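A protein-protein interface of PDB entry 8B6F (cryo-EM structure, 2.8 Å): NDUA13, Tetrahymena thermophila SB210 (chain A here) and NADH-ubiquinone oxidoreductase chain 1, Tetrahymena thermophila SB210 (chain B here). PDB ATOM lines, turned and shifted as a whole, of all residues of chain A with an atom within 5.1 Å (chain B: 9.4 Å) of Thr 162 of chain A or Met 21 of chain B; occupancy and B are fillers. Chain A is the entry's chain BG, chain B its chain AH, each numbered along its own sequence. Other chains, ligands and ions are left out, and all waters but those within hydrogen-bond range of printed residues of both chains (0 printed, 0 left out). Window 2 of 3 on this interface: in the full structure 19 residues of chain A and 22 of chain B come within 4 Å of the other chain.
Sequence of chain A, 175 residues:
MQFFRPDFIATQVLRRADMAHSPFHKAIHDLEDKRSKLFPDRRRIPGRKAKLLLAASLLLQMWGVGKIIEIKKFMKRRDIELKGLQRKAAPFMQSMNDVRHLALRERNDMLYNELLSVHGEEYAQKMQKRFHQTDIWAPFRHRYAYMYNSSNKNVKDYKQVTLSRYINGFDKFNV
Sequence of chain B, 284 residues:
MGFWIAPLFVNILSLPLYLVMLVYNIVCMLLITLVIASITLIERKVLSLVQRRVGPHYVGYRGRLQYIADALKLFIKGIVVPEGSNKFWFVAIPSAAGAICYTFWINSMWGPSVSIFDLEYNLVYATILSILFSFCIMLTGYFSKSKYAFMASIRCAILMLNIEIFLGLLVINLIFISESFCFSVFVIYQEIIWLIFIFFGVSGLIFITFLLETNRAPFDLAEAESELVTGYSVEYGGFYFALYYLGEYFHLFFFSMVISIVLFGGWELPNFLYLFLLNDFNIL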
ATOM      1  N   ASP A 157      -0.513 -19.036   9.703  1.00  0.00           N
ATOM      2  CA  ASP A 157      -0.087 -20.175  10.499  1.00  0.00           C
ATOM      3  C   ASP A 157      -0.747 -20.122  11.875  1.00  0.00           C
ATOM      4  O   ASP A 157      -1.317 -19.108  12.280  1.00  0.00           O
ATOM      5  CB  ASP A 157       1.434 -20.199  10.636  1.00  0.00           C
ATOM      6  CG  ASP A 157       2.137 -20.311   9.298  1.00  0.00           C
ATOM      7  OD1 ASP A 157       1.526 -20.844   8.349  1.00  0.00           O
ATOM      8  OD2 ASP A 157       3.301 -19.868   9.196  1.00  0.00           O
ATOM      9  N   TYR A 158      -0.660 -21.233  12.607  1.00  0.00           N
ATOM     10  CA  TYR A 158      -1.238 -21.263  13.947  1.00  0.00           C
ATOM     11  C   TYR A 158      -0.541 -20.266  14.862  1.00  0.00           C
ATOM     12  O   TYR A 158      -1.191 -19.591  15.668  1.00  0.00           O
ATOM     13  CB  TYR A 158      -1.165 -22.677  14.523  1.00  0.00           C
ATOM     14  CG  TYR A 158      -2.082 -23.651  13.827  1.00  0.00           C
ATOM     15  CD1 TYR A 158      -3.428 -23.709  14.157  1.00  0.00           C
ATOM     16  CD2 TYR A 158      -1.609 -24.508  12.844  1.00  0.00           C
ATOM     17  CE1 TYR A 158      -4.278 -24.590  13.532  1.00  0.00           C
ATOM     18  CE2 TYR A 158      -2.455 -25.397  12.209  1.00  0.00           C
ATOM     19  CZ  TYR A 158      -3.790 -25.430  12.560  1.00  0.00           C
ATOM     20  OH  TYR A 158      -4.651 -26.304  11.946  1.00  0.00           O
ATOM     21  N   LYS A 159       0.783 -20.162  14.755  1.00  0.00           N
ATOM     22  CA  LYS A 159       1.518 -19.200  15.570  1.00  0.00           C
ATOM     23  C   LYS A 159       1.060 -17.777  15.279  1.00  0.00           C
ATOM     24  O   LYS A 159       0.836 -16.985  16.200  1.00  0.00           O
ATOM     25  CB  LYS A 159       3.013 -19.336  15.295  1.00  0.00           C
ATOM     26  CG  LYS A 159       3.876 -18.306  15.998  1.00  0.00           C
ATOM     27  CD  LYS A 159       5.323 -18.552  15.649  1.00  0.00           C
ATOM     28  CE  LYS A 159       6.256 -17.543  16.269  1.00  0.00           C
ATOM     29  NZ  LYS A 159       7.639 -17.905  15.855  1.00  0.00           N
ATOM     30  N   GLN A 160       0.919 -17.435  13.998  1.00  0.00           N
ATOM     31  CA  GLN A 160       0.444 -16.104  13.639  1.00  0.00           C
ATOM     32  C   GLN A 160      -0.976 -15.875  14.136  1.00  0.00           C
ATOM     33  O   GLN A 160      -1.295 -14.797  14.650  1.00  0.00           O
ATOM     34  CB  GLN A 160       0.513 -15.911  12.127  1.00  0.00           C
ATOM     35  CG  GLN A 160       1.914 -16.006  11.552  1.00  0.00           C
ATOM     36  CD  GLN A 160       1.938 -15.789  10.052  1.00  0.00           C
ATOM     37  OE1 GLN A 160       2.577 -16.540   9.317  1.00  0.00           O
ATOM     38  NE2 GLN A 160       1.249 -14.752   9.590  1.00  0.00           N
ATOM     39  N   VAL A 161      -1.843 -16.876  13.986  1.00  0.00           N
ATOM     40  CA  VAL A 161      -3.222 -16.735  14.443  1.00  0.00           C
ATOM     41  C   VAL A 161      -3.256 -16.437  15.935  1.00  0.00           C
ATOM     42  O   VAL A 161      -4.032 -15.591  16.395  1.00  0.00           O
ATOM     43  CB  VAL A 161      -4.022 -18.007  14.100  1.00  0.00           C
ATOM     44  CG1 VAL A 161      -5.340 -18.052  14.861  1.00  0.00           C
ATOM     45  CG2 VAL A 161      -4.278 -18.079  12.606  1.00  0.00           C
ATOM     46  N   THR A 162      -2.426 -17.129  16.715  1.00  0.00           N
ATOM     47  CA  THR A 162      -2.415 -16.899  18.155  1.00  0.00           C
ATOM     48  C   THR A 162      -1.851 -15.523  18.492  1.00  0.00           C
ATOM     49  O   THR A 162      -2.431 -14.783  19.294  1.00  0.00           O
ATOM     50  CB  THR A 162      -1.603 -17.996  18.847  1.00  0.00           C
ATOM     51  OG1 THR A 162      -2.168 -19.278  18.543  1.00  0.00           O
ATOM     52  CG2 THR A 162      -1.603 -17.800  20.355  1.00  0.00           C
ATOM     53  N   LEU A 163      -0.721 -15.160  17.883  1.00  0.00           N
ATOM     54  CA  LEU A 163      -0.007 -13.958  18.302  1.00  0.00           C
ATOM     55  C   LEU A 163      -0.665 -12.684  17.791  1.00  0.00           C
ATOM     56  O   LEU A 163      -0.712 -11.681  18.510  1.00  0.00           O
ATOM     57  CB  LEU A 163       1.448 -14.024  17.834  1.00  0.00           C
ATOM     58  CG  LEU A 163       2.324 -15.093  18.493  1.00  0.00           C
ATOM     59  CD1 LEU A 163       3.731 -15.044  17.920  1.00  0.00           C
ATOM     60  CD2 LEU A 163       2.361 -14.941  20.009  1.00  0.00           C
ATOM     61  N   SER A 164      -1.173 -12.693  16.559  1.00  0.00           N
ATOM     62  CA  SER A 164      -1.647 -11.454  15.955  1.00  0.00           C
ATOM     63  C   SER A 164      -2.795 -10.828  16.735  1.00  0.00           C
ATOM     64  O   SER A 164      -3.071  -9.638  16.555  1.00  0.00           O
ATOM     65  CB  SER A 164      -2.083 -11.706  14.513  1.00  0.00           C
ATOM     66  OG  SER A 164      -3.070 -12.717  14.453  1.00  0.00           O
ATOM     67  N   ARG A 165      -3.477 -11.598  17.583  1.00  0.00           N
ATOM     68  CA  ARG A 165      -4.548 -11.036  18.395  1.00  0.00           C
ATOM     69  C   ARG A 165      -4.026 -10.190  19.549  1.00  0.00           C
ATOM     70  O   ARG A 165      -4.811  -9.456  20.158  1.00  0.00           O
ATOM     71  CB  ARG A 165      -5.435 -12.163  18.935  1.00  0.00           C
ATOM     72  CG  ARG A 165      -6.764 -11.700  19.527  1.00  0.00           C
ATOM     73  CD  ARG A 165      -7.665 -11.073  18.472  1.00  0.00           C
ATOM     74  NE  ARG A 165      -8.976 -10.727  19.007  1.00  0.00           N
ATOM     75  CZ  ARG A 165      -9.924 -10.102  18.322  1.00  0.00           C
ATOM     76  NH1 ARG A 165      -9.741  -9.734  17.065  1.00  0.00           N
ATOM     77  NH2 ARG A 165     -11.087  -9.842  18.913  1.00  0.00           N
ATOM     78  N   TYR A 166      -2.732 -10.269  19.858  1.00  0.00           N
ATOM     79  CA  TYR A 166      -2.139  -9.508  20.951  1.00  0.00           C
ATOM     80  C   TYR A 166      -0.913  -8.700  20.557  1.00  0.00           C
ATOM     81  O   TYR A 166      -0.557  -7.771  21.293  1.00  0.00           O
ATOM     82  CB  TYR A 166      -1.745 -10.445  22.104  1.00  0.00           C
ATOM     83  CG  TYR A 166      -2.909 -11.195  22.703  1.00  0.00           C
ATOM     84  CD1 TYR A 166      -3.394 -12.350  22.107  1.00  0.00           C
ATOM     85  CD2 TYR A 166      -3.521 -10.750  23.867  1.00  0.00           C
ATOM     86  CE1 TYR A 166      -4.458 -13.040  22.650  1.00  0.00           C
ATOM     87  CE2 TYR A 166      -4.585 -11.434  24.417  1.00  0.00           C
ATOM     88  CZ  TYR A 166      -5.051 -12.575  23.802  1.00  0.00           C
ATOM     89  OH  TYR A 166      -6.109 -13.263  24.345  1.00  0.00           O
ATOM     90  N   SER B  14      10.333 -15.143  20.186  1.00  0.00           N
ATOM     91  CA  SER B  14       8.880 -15.174  20.258  1.00  0.00           C
ATOM     92  C   SER B  14       8.344 -15.421  21.657  1.00  0.00           C
ATOM     93  O   SER B  14       7.189 -15.080  21.929  1.00  0.00           O
ATOM     94  CB  SER B  14       8.330 -16.253  19.329  1.00  0.00           C
ATOM     95  OG  SER B  14       8.666 -15.940  17.999  1.00  0.00           O
ATOM     96  N   LEU B  15       9.144 -16.009  22.540  1.00  0.00           N
ATOM     97  CA  LEU B  15       8.675 -16.249  23.899  1.00  0.00           C
ATOM     98  C   LEU B  15       8.218 -14.968  24.579  1.00  0.00           C
ATOM     99  O   LEU B  15       7.191 -15.008  25.278  1.00  0.00           O
ATOM    100  CB  LEU B  15       9.777 -16.943  24.707  1.00  0.00           C
ATOM    101  CG  LEU B  15      10.318 -18.239  24.096  1.00  0.00           C
ATOM    102  CD1 LEU B  15      11.404 -18.826  24.981  1.00  0.00           C
ATOM    103  CD2 LEU B  15       9.205 -19.253  23.871  1.00  0.00           C
ATOM    104  N   PRO B  16       8.900 -13.830  24.438  1.00  0.00           N
ATOM    105  CA  PRO B  16       8.374 -12.603  25.050  1.00  0.00           C
ATOM    106  C   PRO B  16       6.969 -12.261  24.589  1.00  0.00           C
ATOM    107  O   PRO B  16       6.188 -11.713  25.375  1.00  0.00           O
ATOM    108  CB  PRO B  16       9.383 -11.534  24.607  1.00  0.00           C
ATOM    109  CG  PRO B  16      10.634 -12.280  24.328  1.00  0.00           C
ATOM    110  CD  PRO B  16      10.202 -13.606  23.787  1.00  0.00           C
ATOM    111  N   LEU B  17       6.619 -12.576  23.338  1.00  0.00           N
ATOM    112  CA  LEU B  17       5.262 -12.320  22.865  1.00  0.00           C
ATOM    113  C   LEU B  17       4.242 -13.171  23.611  1.00  0.00           C
ATOM    114  O   LEU B  17       3.173 -12.678  23.989  1.00  0.00           O
ATOM    115  CB  LEU B  17       5.175 -12.571  21.361  1.00  0.00           C
ATOM    116  CG  LEU B  17       6.201 -11.829  20.501  1.00  0.00           C
ATOM    117  CD1 LEU B  17       5.876 -12.009  19.033  1.00  0.00           C
ATOM    118  CD2 LEU B  17       6.263 -10.350  20.854  1.00  0.00           C
ATOM    119  N   TYR B  18       4.549 -14.450  23.832  1.00  0.00           N
ATOM    120  CA  TYR B  18       3.659 -15.288  24.626  1.00  0.00           C
ATOM    121  C   TYR B  18       3.559 -14.770  26.052  1.00  0.00           C
ATOM    122  O   TYR B  18       2.489 -14.820  26.668  1.00  0.00           O
ATOM    123  CB  TYR B  18       4.144 -16.737  24.611  1.00  0.00           C
ATOM    124  CG  TYR B  18       4.040 -17.397  23.258  1.00  0.00           C
ATOM    125  CD1 TYR B  18       2.864 -18.017  22.857  1.00  0.00           C
ATOM    126  CD2 TYR B  18       5.114 -17.400  22.379  1.00  0.00           C
ATOM    127  CE1 TYR B  18       2.760 -18.621  21.621  1.00  0.00           C
ATOM    128  CE2 TYR B  18       5.021 -18.001  21.142  1.00  0.00           C
ATOM    129  CZ  TYR B  18       3.842 -18.610  20.767  1.00  0.00           C
ATOM    130  OH  TYR B  18       3.745 -19.212  19.535  1.00  0.00           O
ATOM    131  N   LEU B  19       4.671 -14.277  26.599  1.00  0.00           N
ATOM    132  CA  LEU B  19       4.638 -13.695  27.934  1.00  0.00           C
ATOM    133  C   LEU B  19       3.731 -12.470  27.970  1.00  0.00           C
ATOM    134  O   LEU B  19       2.969 -12.281  28.923  1.00  0.00           O
ATOM    135  CB  LEU B  19       6.054 -13.334  28.379  1.00  0.00           C
ATOM    136  CG  LEU B  19       6.215 -12.845  29.820  1.00  0.00           C
ATOM    137  CD1 LEU B  19       5.776 -13.914  30.808  1.00  0.00           C
ATOM    138  CD2 LEU B  19       7.653 -12.433  30.084  1.00  0.00           C
ATOM    139  N   VAL B  20       3.784 -11.637  26.928  1.00  0.00           N
ATOM    140  CA  VAL B  20       2.922 -10.459  26.869  1.00  0.00           C
ATOM    141  C   VAL B  20       1.461 -10.877  26.787  1.00  0.00           C
ATOM    142  O   VAL B  20       0.594 -10.292  27.448  1.00  0.00           O
ATOM    143  CB  VAL B  20       3.326  -9.562  25.683  1.00  0.00           C
ATOM    144  CG1 VAL B  20       2.263  -8.504  25.408  1.00  0.00           C
ATOM    145  CG2 VAL B  20       4.664  -8.905  25.954  1.00  0.00           C
ATOM    146  N   MET B  21       1.162 -11.891  25.975  1.00  0.00           N
ATOM    147  CA  MET B  21      -0.201 -12.403  25.903  1.00  0.00           C
ATOM    148  C   MET B  21      -0.667 -12.887  27.269  1.00  0.00           C
ATOM    149  O   MET B  21      -1.791 -12.597  27.692  1.00  0.00           O
ATOM    150  CB  MET B  21      -0.274 -13.526  24.869  1.00  0.00           C
ATOM    151  CG  MET B  21      -1.609 -14.250  24.814  1.00  0.00           C
ATOM    152  SD  MET B  21      -1.622 -15.540  23.557  1.00  0.00           S
ATOM    153  CE  MET B  21      -3.223 -16.279  23.853  1.00  0.00           C
ATOM    154  N   LEU B  22       0.189 -13.627  27.975  1.00  0.00           N
ATOM    155  CA  LEU B  22      -0.157 -14.086  29.315  1.00  0.00           C
ATOM    156  C   LEU B  22      -0.408 -12.911  30.252  1.00  0.00           C
ATOM    157  O   LEU B  22      -1.356 -12.932  31.046  1.00  0.00           O
ATOM    158  CB  LEU B  22       0.960 -14.974  29.859  1.00  0.00           C
ATOM    159  CG  LEU B  22       0.835 -15.426  31.314  1.00  0.00           C
ATOM    160  CD1 LEU B  22      -0.417 -16.267  31.516  1.00  0.00           C
ATOM    161  CD2 LEU B  22       2.080 -16.187  31.721  1.00  0.00           C
ATOM    162  N   VAL B  23       0.426 -11.875  30.173  1.00  0.00           N
ATOM    163  CA  VAL B  23       0.265 -10.719  31.051  1.00  0.00           C
ATOM    164  C   VAL B  23      -1.064 -10.028  30.789  1.00  0.00           C
ATOM    165  O   VAL B  23      -1.782  -9.657  31.725  1.00  0.00           O
ATOM    166  CB  VAL B  23       1.451  -9.753  30.876  1.00  0.00           C
ATOM    167  CG1 VAL B  23       1.194  -8.438  31.601  1.00  0.00           C
ATOM    168  CG2 VAL B  23       2.720 -10.386  31.395  1.00  0.00           C
ATOM    169  N   TYR B  24      -1.421  -9.850  29.515  1.00  0.00           N
ATOM    170  CA  TYR B  24      -2.692  -9.207  29.199  1.00  0.00           C
ATOM    171  C   TYR B  24      -3.866 -10.037  29.701  1.00  0.00           C
ATOM    172  O   TYR B  24      -4.832  -9.491  30.243  1.00  0.00           O
ATOM    173  CB  TYR B  24      -2.800  -8.972  27.693  1.00  0.00           C
ATOM    174  CG  TYR B  24      -1.882  -7.892  27.158  1.00  0.00           C
ATOM    175  CD1 TYR B  24      -1.162  -7.064  28.014  1.00  0.00           C
ATOM    176  CD2 TYR B  24      -1.746  -7.693  25.792  1.00  0.00           C
ATOM    177  CE1 TYR B  24      -0.332  -6.078  27.524  1.00  0.00           C
ATOM    178  CE2 TYR B  24      -0.918  -6.709  25.292  1.00  0.00           C
ATOM    179  CZ  TYR B  24      -0.214  -5.905  26.163  1.00  0.00           C
ATOM    180  OH  TYR B  24       0.610  -4.925  25.669  1.00  0.00           O
ATOM    181  N   ASN B  25      -3.810 -11.357  29.518  1.00  0.00           N
ATOM    182  CA  ASN B  25      -4.880 -12.206  30.029  1.00  0.00           C
ATOM    183  C   ASN B  25      -4.961 -12.122  31.547  1.00  0.00           C
ATOM    184  O   ASN B  25      -6.056 -12.106  32.118  1.00  0.00           O
ATOM    185  CB  ASN B  25      -4.671 -13.652  29.584  1.00  0.00           C
ATOM    186  CG  ASN B  25      -4.724 -13.810  28.082  1.00  0.00           C
ATOM    187  OD1 ASN B  25      -3.830 -14.394  27.473  1.00  0.00           O
ATOM    188  ND2 ASN B  25      -5.777 -13.287  27.473  1.00  0.00           N
ATOM    189  N   ILE B  26      -3.809 -12.074  32.218  1.00  0.00           N
ATOM    190  CA  ILE B  26      -3.803 -11.948  33.672  1.00  0.00           C
ATOM    191  C   ILE B  26      -4.453 -10.637  34.092  1.00  0.00           C
ATOM    192  O   ILE B  26      -5.238 -10.594  35.047  1.00  0.00           O
ATOM    193  CB  ILE B  26      -2.363 -12.068  34.212  1.00  0.00           C
ATOM    194  CG1 ILE B  26      -1.823 -13.486  33.997  1.00  0.00           C
ATOM    195  CG2 ILE B  26      -2.298 -11.666  35.688  1.00  0.00           C
ATOM    196  CD1 ILE B  26      -2.390 -14.525  34.931  1.00  0.00           C
ATOM    197  N   VAL B  27      -4.139  -9.547  33.389  1.00  0.00           N
ATOM    198  CA  VAL B  27      -4.735  -8.257  33.724  1.00  0.00           C
ATOM    199  C   VAL B  27      -6.247  -8.307  33.551  1.00  0.00           C
ATOM    200  O   VAL B  27      -6.999  -7.828  34.408  1.00  0.00           O
ATOM    201  CB  VAL B  27      -4.101  -7.142  32.872  1.00  0.00           C
ATOM    202  CG1 VAL B  27      -4.883  -5.842  33.006  1.00  0.00           C
ATOM    203  CG2 VAL B  27      -2.655  -6.930  33.271  1.00  0.00           C
ATOM    204  N   CYS B  28      -6.720  -8.883  32.443  1.00  0.00           N
ATOM    205  CA  CYS B  28      -8.162  -8.969  32.229  1.00  0.00           C
ATOM    206  C   CYS B  28      -8.830  -9.783  33.329  1.00  0.00           C
ATOM    207  O   CYS B  28      -9.884  -9.396  33.847  1.00  0.00           O
ATOM    208  CB  CYS B  28      -8.454  -9.583  30.862  1.00  0.00           C
ATOM    209  SG  CYS B  28      -8.006  -8.537  29.463  1.00  0.00           S
ATOM    210  N   MET B  29      -8.233 -10.918  33.698  1.00  0.00           N
ATOM    211  CA  MET B  29      -8.821 -11.757  34.735  1.00  0.00           C
ATOM    212  C   MET B  29      -8.828 -11.050  36.085  1.00  0.00           C
ATOM    213  O   MET B  29      -9.792 -11.168  36.849  1.00  0.00           O
ATOM    214  CB  MET B  29      -8.072 -13.086  34.816  1.00  0.00           C
ATOM    215  CG  MET B  29      -8.411 -14.026  33.668  1.00  0.00           C
ATOM    216  SD  MET B  29      -7.568 -15.614  33.748  1.00  0.00           S
ATOM    217  CE  MET B  29      -5.922 -15.142  33.234  1.00  0.00           C
ATOM    218  N   TRP B 105     -15.230 -15.272  30.976  1.00  0.00           N
ATOM    219  CA  TRP B 105     -15.214 -13.908  30.463  1.00  0.00           C
ATOM    220  C   TRP B 105     -14.845 -13.817  28.989  1.00  0.00           C
ATOM    221  O   TRP B 105     -15.034 -12.752  28.394  1.00  0.00           O
ATOM    222  CB  TRP B 105     -14.245 -13.050  31.279  1.00  0.00           C
ATOM    223  CG  TRP B 105     -12.802 -13.378  31.056  1.00  0.00           C
ATOM    224  CD1 TRP B 105     -12.049 -14.264  31.761  1.00  0.00           C
ATOM    225  CD2 TRP B 105     -11.936 -12.818  30.062  1.00  0.00           C
ATOM    226  NE1 TRP B 105     -10.767 -14.295  31.269  1.00  0.00           N
ATOM    227  CE2 TRP B 105     -10.673 -13.416  30.224  1.00  0.00           C
ATOM    228  CE3 TRP B 105     -12.110 -11.870  29.049  1.00  0.00           C
ATOM    229  CZ2 TRP B 105      -9.586 -13.098  29.412  1.00  0.00           C
ATOM    230  CZ3 TRP B 105     -11.029 -11.554  28.243  1.00  0.00           C
ATOM    231  CH2 TRP B 105      -9.782 -12.167  28.430  1.00  0.00           C
ATOM    232  N   ILE B 116     -12.477 -10.170  23.079  1.00  0.00           N
ATOM    233  CA  ILE B 116     -11.096 -10.639  23.147  1.00  0.00           C
ATOM    234  C   ILE B 116     -10.805 -11.601  22.002  1.00  0.00           C
ATOM    235  O   ILE B 116      -9.707 -11.599  21.435  1.00  0.00           O
ATOM    236  CB  ILE B 116     -10.817 -11.279  24.521  1.00  0.00           C
ATOM    237  CG1 ILE B 116      -9.329 -11.607  24.676  1.00  0.00           C
ATOM    238  CG2 ILE B 116     -11.658 -12.534  24.722  1.00  0.00           C
ATOM    239  CD1 ILE B 116      -8.424 -10.393  24.677  1.00  0.00           C
ATOM    240  N   PHE B 117     -11.781 -12.430  21.646  1.00  0.00           N
ATOM    241  CA  PHE B 117     -11.659 -13.368  20.542  1.00  0.00           C
ATOM    242  C   PHE B 117     -12.826 -13.177  19.585  1.00  0.00           C
ATOM    243  O   PHE B 117     -13.901 -12.714  19.975  1.00  0.00           O
ATOM    244  CB  PHE B 117     -11.627 -14.818  21.036  1.00  0.00           C
ATOM    245  CG  PHE B 117     -10.491 -15.124  21.962  1.00  0.00           C
ATOM    246  CD1 PHE B 117      -9.271 -14.480  21.837  1.00  0.00           C
ATOM    247  CD2 PHE B 117     -10.646 -16.063  22.964  1.00  0.00           C
ATOM    248  CE1 PHE B 117      -8.230 -14.768  22.695  1.00  0.00           C
ATOM    249  CE2 PHE B 117      -9.611 -16.356  23.823  1.00  0.00           C
ATOM    250  CZ  PHE B 117      -8.401 -15.708  23.690  1.00  0.00           C
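Of the 10 printed residues of chain A, 5 touch a printed residue of chain B.
Printed residues of chain A that touch a printed residue of chain B: Lys 159, Thr 162, Leu 163, Arg 165 and Tyr 166.
Hydrophobic or aromatic side chains of chain A that line the printed part of chain B: Leu 163 and Tyr 166.
Of the 19 printed residues of chain B, 7 touch a printed residue of chain A.
Among the printed residues, 10 pairs touch across the chains.
Among the printed residues, no Asp or Glu carboxylate lies within 4 Å of a Lys or Arg side-chain nitrogen of the other chain.
Lys 159 of chain A touches Tyr 18 of chain B.
Met 21 of chain B touches Thr 162 of chain A (SD to CG2, 3.9 Å).
CD1 of Leu 163 of chain A touches CD1 of Leu 17 of chain B (3.9 Å).
Arg 165 of chain A touches Phe 117 of chain B.
Tyr 166 of chain A touches Met 21 of chain B (CE1 to CE, 3.7 Å).
OH of Tyr 166 of chain A touches CG1 of Ile 116 of chain B (3.6 Å).
Tyr 166 of chain A touches Phe 117 of chain B (OH to CE1, 3.1 Å).
Met 21 of chain B touches two residues of chain A.
No residue of chain B comes within 4 Å of Val 161 of chain A.
Printed residues of chain A within 4 Å of Asn 25 of chain B: Tyr 166 (3.1 Å).
Of the printed residues of chain A, Tyr 18 of chain B touches Lys 159.
Of the printed residues of chain A, Leu 17 of chain B touches Leu 163 (3.9 Å).
Printed residues of chain B within 4 Å of Lys 159 of chain A: Ser 14 (3.1 Å) and Tyr 18 (3.7 Å).
Of the printed residues of chain A, Phe 117 of chain B touches Arg 165 and Tyr 166.
The nearest residue of chain B that does not touch Thr 162 of chain A is Tyr 18 of chain B (4.6 Å).
The nearest printed residue of chain A that does not touch Met 21 of chain B is Leu 163 of chain A (5.4 Å).
O of Tyr 158 of chain A lies within hydrogen-bond range of OG1 of Thr 162 of chain A (3.1 Å).
O of Met 21 of chain B sits close to OD1 of Asn 25 of chain B (2.7 Å).
OG of Ser 14 of chain B lies within hydrogen-bond range of NZ of Lys 159 of chain A (3.1 Å).
The backbone carbonyl oxygen (O) of Ile 116 of chain B sits at hydrogen-bond distance from the guanidinium group (NE) of Arg 165 of chain A, 2.7 Å away.
ND2 of Asn 25 of chain B is in hydrogen-bond range of OH of Tyr 166 of chain A (3.1 Å).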
